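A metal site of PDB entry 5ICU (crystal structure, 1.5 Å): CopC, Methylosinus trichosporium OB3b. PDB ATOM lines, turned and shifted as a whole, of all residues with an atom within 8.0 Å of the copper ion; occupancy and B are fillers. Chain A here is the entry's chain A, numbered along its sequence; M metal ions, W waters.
OG of Ser 81 sits at hydrogen-bond distance from O of His 85, at 2.8 Å.
Within 4 Å of the copper ion: His 1, Asp 83 and His 85.
ND1 of His 85 binds the copper ion (2.0 Å). N of His 1 is bound to the copper ion (2.0 Å). ND1 of His 1 binds the copper ion, 2.1 Å away. OD2 of Asp 83 is bound to the copper ion (2.3 Å). The copper ion is bound by water W1, 2.4 Å away.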
ATOM      1  N   HIS A   1      21.277 -26.821  -4.268  1.00  0.00           N
ATOM      2  CA  HIS A   1      22.452 -26.243  -3.592  1.00  0.00           C
ATOM      3  C   HIS A   1      22.612 -24.814  -4.001  1.00  0.00           C
ATOM      4  O   HIS A   1      22.564 -24.495  -5.201  1.00  0.00           O
ATOM      5  CB  HIS A   1      23.714 -26.968  -4.013  1.00  0.00           C
ATOM      6  CG  HIS A   1      23.806 -28.369  -3.522  1.00  0.00           C
ATOM      7  ND1 HIS A   1      22.742 -29.240  -3.502  1.00  0.00           N
ATOM      8  CD2 HIS A   1      24.830 -29.019  -2.955  1.00  0.00           C
ATOM      9  CE1 HIS A   1      23.143 -30.409  -3.039  1.00  0.00           C
ATOM     10  NE2 HIS A   1      24.412 -30.302  -2.707  1.00  0.00           N
ATOM     11  N   SER A   2      22.805 -23.942  -3.014  1.00  0.00           N
ATOM     12  CA  SER A   2      23.045 -22.523  -3.239  1.00  0.00           C
ATOM     13  C   SER A   2      24.509 -22.280  -3.148  1.00  0.00           C
ATOM     14  O   SER A   2      25.060 -22.081  -2.090  1.00  0.00           O
ATOM     15  CB  SER A   2      22.276 -21.721  -2.211  1.00  0.00           C
ATOM     16  OG  SER A   2      20.893 -21.882  -2.475  1.00  0.00           O
ATOM     17  N   PHE A   3      25.193 -22.413  -4.273  1.00  0.00           N
ATOM     18  CA  PHE A   3      26.650 -22.254  -4.326  1.00  0.00           C
ATOM     19  C   PHE A   3      27.083 -20.800  -4.275  1.00  0.00           C
ATOM     20  O   PHE A   3      26.383 -19.930  -4.773  1.00  0.00           O
ATOM     21  CB  PHE A   3      27.181 -22.891  -5.606  1.00  0.00           C
ATOM     22  CG  PHE A   3      27.087 -24.412  -5.621  1.00  0.00           C
ATOM     23  CD1 PHE A   3      27.778 -25.148  -4.674  1.00  0.00           C
ATOM     24  CD2 PHE A   3      26.301 -25.099  -6.533  1.00  0.00           C
ATOM     25  CE1 PHE A   3      27.692 -26.533  -4.653  1.00  0.00           C
ATOM     26  CE2 PHE A   3      26.225 -26.503  -6.511  1.00  0.00           C
ATOM     27  CZ  PHE A   3      26.959 -27.191  -5.542  1.00  0.00           C
ATOM     28  N   SER A  81      20.947 -24.094   2.310  1.00  0.00           N
ATOM     29  CA  SER A  81      20.242 -23.638   1.094  1.00  0.00           C
ATOM     30  C   SER A  81      18.742 -23.751   1.270  1.00  0.00           C
ATOM     31  O   SER A  81      18.254 -24.582   2.016  1.00  0.00           O
ATOM     32  CB  SER A  81      20.667 -24.475  -0.104  1.00  0.00           C
ATOM     33  OG  SER A  81      22.081 -24.555  -0.267  1.00  0.00           O
ATOM     34  N   SER A  82      18.013 -22.959   0.496  1.00  0.00           N
ATOM     35  CA  SER A  82      16.556 -22.970   0.586  1.00  0.00           C
ATOM     36  C   SER A  82      16.013 -24.296   0.100  1.00  0.00           C
ATOM     37  O   SER A  82      14.877 -24.649   0.491  1.00  0.00           O
ATOM     38  CB  SER A  82      15.946 -21.783  -0.151  1.00  0.00           C
ATOM     39  OG  SER A  82      16.352 -20.550   0.449  1.00  0.00           O
ATOM     40  N   ASP A  83      16.771 -25.084  -0.681  1.00  0.00           N
ATOM     41  CA  ASP A  83      16.287 -26.372  -1.125  1.00  0.00           C
ATOM     42  C   ASP A  83      16.619 -27.480  -0.156  1.00  0.00           C
ATOM     43  O   ASP A  83      16.428 -28.678  -0.488  1.00  0.00           O
ATOM     44  CB  ASP A  83      16.806 -26.682  -2.534  1.00  0.00           C
ATOM     45  CG  ASP A  83      18.274 -27.078  -2.556  1.00  0.00           C
ATOM     46  OD1 ASP A  83      19.008 -26.814  -1.565  1.00  0.00           O
ATOM     47  OD2 ASP A  83      18.710 -27.614  -3.616  1.00  0.00           O
ATOM     48  N   GLY A  84      17.111 -27.132   1.044  1.00  0.00           N
ATOM     49  CA  GLY A  84      17.401 -28.061   2.090  1.00  0.00           C
ATOM     50  C   GLY A  84      18.806 -28.610   2.142  1.00  0.00           C
ATOM     51  O   GLY A  84      19.080 -29.466   2.950  1.00  0.00           O
ATOM     52  N   HIS A  85      19.724 -28.166   1.262  1.00  0.00           N
ATOM     53  CA  HIS A  85      21.079 -28.761   1.146  1.00  0.00           C
ATOM     54  C   HIS A  85      22.135 -27.859   1.696  1.00  0.00           C
ATOM     55  O   HIS A  85      22.076 -26.642   1.536  1.00  0.00           O
ATOM     56  CB  HIS A  85      21.359 -29.095  -0.314  1.00  0.00           C
ATOM     57  CG  HIS A  85      20.299 -29.968  -0.922  1.00  0.00           C
ATOM     58  ND1 HIS A  85      19.964 -29.882  -2.237  1.00  0.00           N
ATOM     59  CD2 HIS A  85      19.434 -30.851  -0.379  1.00  0.00           C
ATOM     60  CE1 HIS A  85      18.951 -30.699  -2.497  1.00  0.00           C
ATOM     61  NE2 HIS A  85      18.621 -31.306  -1.380  1.00  0.00           N
ATOM     62  N   ILE A  86      23.073 -28.464   2.399  1.00  0.00           N
ATOM     63  CA  ILE A  86      24.145 -27.719   3.038  1.00  0.00           C
ATOM     64  C   ILE A  86      25.300 -27.523   2.062  1.00  0.00           C
ATOM     65  O   ILE A  86      25.687 -28.455   1.353  1.00  0.00           O
ATOM     66  CB  ILE A  86      24.642 -28.465   4.290  1.00  0.00           C
ATOM     67  CG1 ILE A  86      23.481 -28.674   5.264  1.00  0.00           C
ATOM     68  CG2 ILE A  86      25.804 -27.744   4.945  1.00  0.00           C
ATOM     69  CD1 ILE A  86      23.749 -29.740   6.304  1.00  0.00           C
ATOM     70  N   VAL A  87      25.826 -26.302   2.046  1.00  0.00           N
ATOM     71  CA  VAL A  87      26.983 -25.934   1.244  1.00  0.00           C
ATOM     72  C   VAL A  87      28.076 -25.338   2.144  1.00  0.00           C
ATOM     73  O   VAL A  87      27.816 -24.393   2.918  1.00  0.00           O
ATOM     74  CB  VAL A  87      26.595 -24.922   0.142  1.00  0.00           C
ATOM     75  CG1 VAL A  87      27.823 -24.360  -0.536  1.00  0.00           C
ATOM     76  CG2 VAL A  87      25.621 -25.544  -0.863  1.00  0.00           C
HETATM   77 CU    CU M   1      20.767 -28.649  -3.541  1.00  0.00          CU
HETATM   78  O   HOH W   1      20.154 -29.688  -5.583  1.00  0.00           O
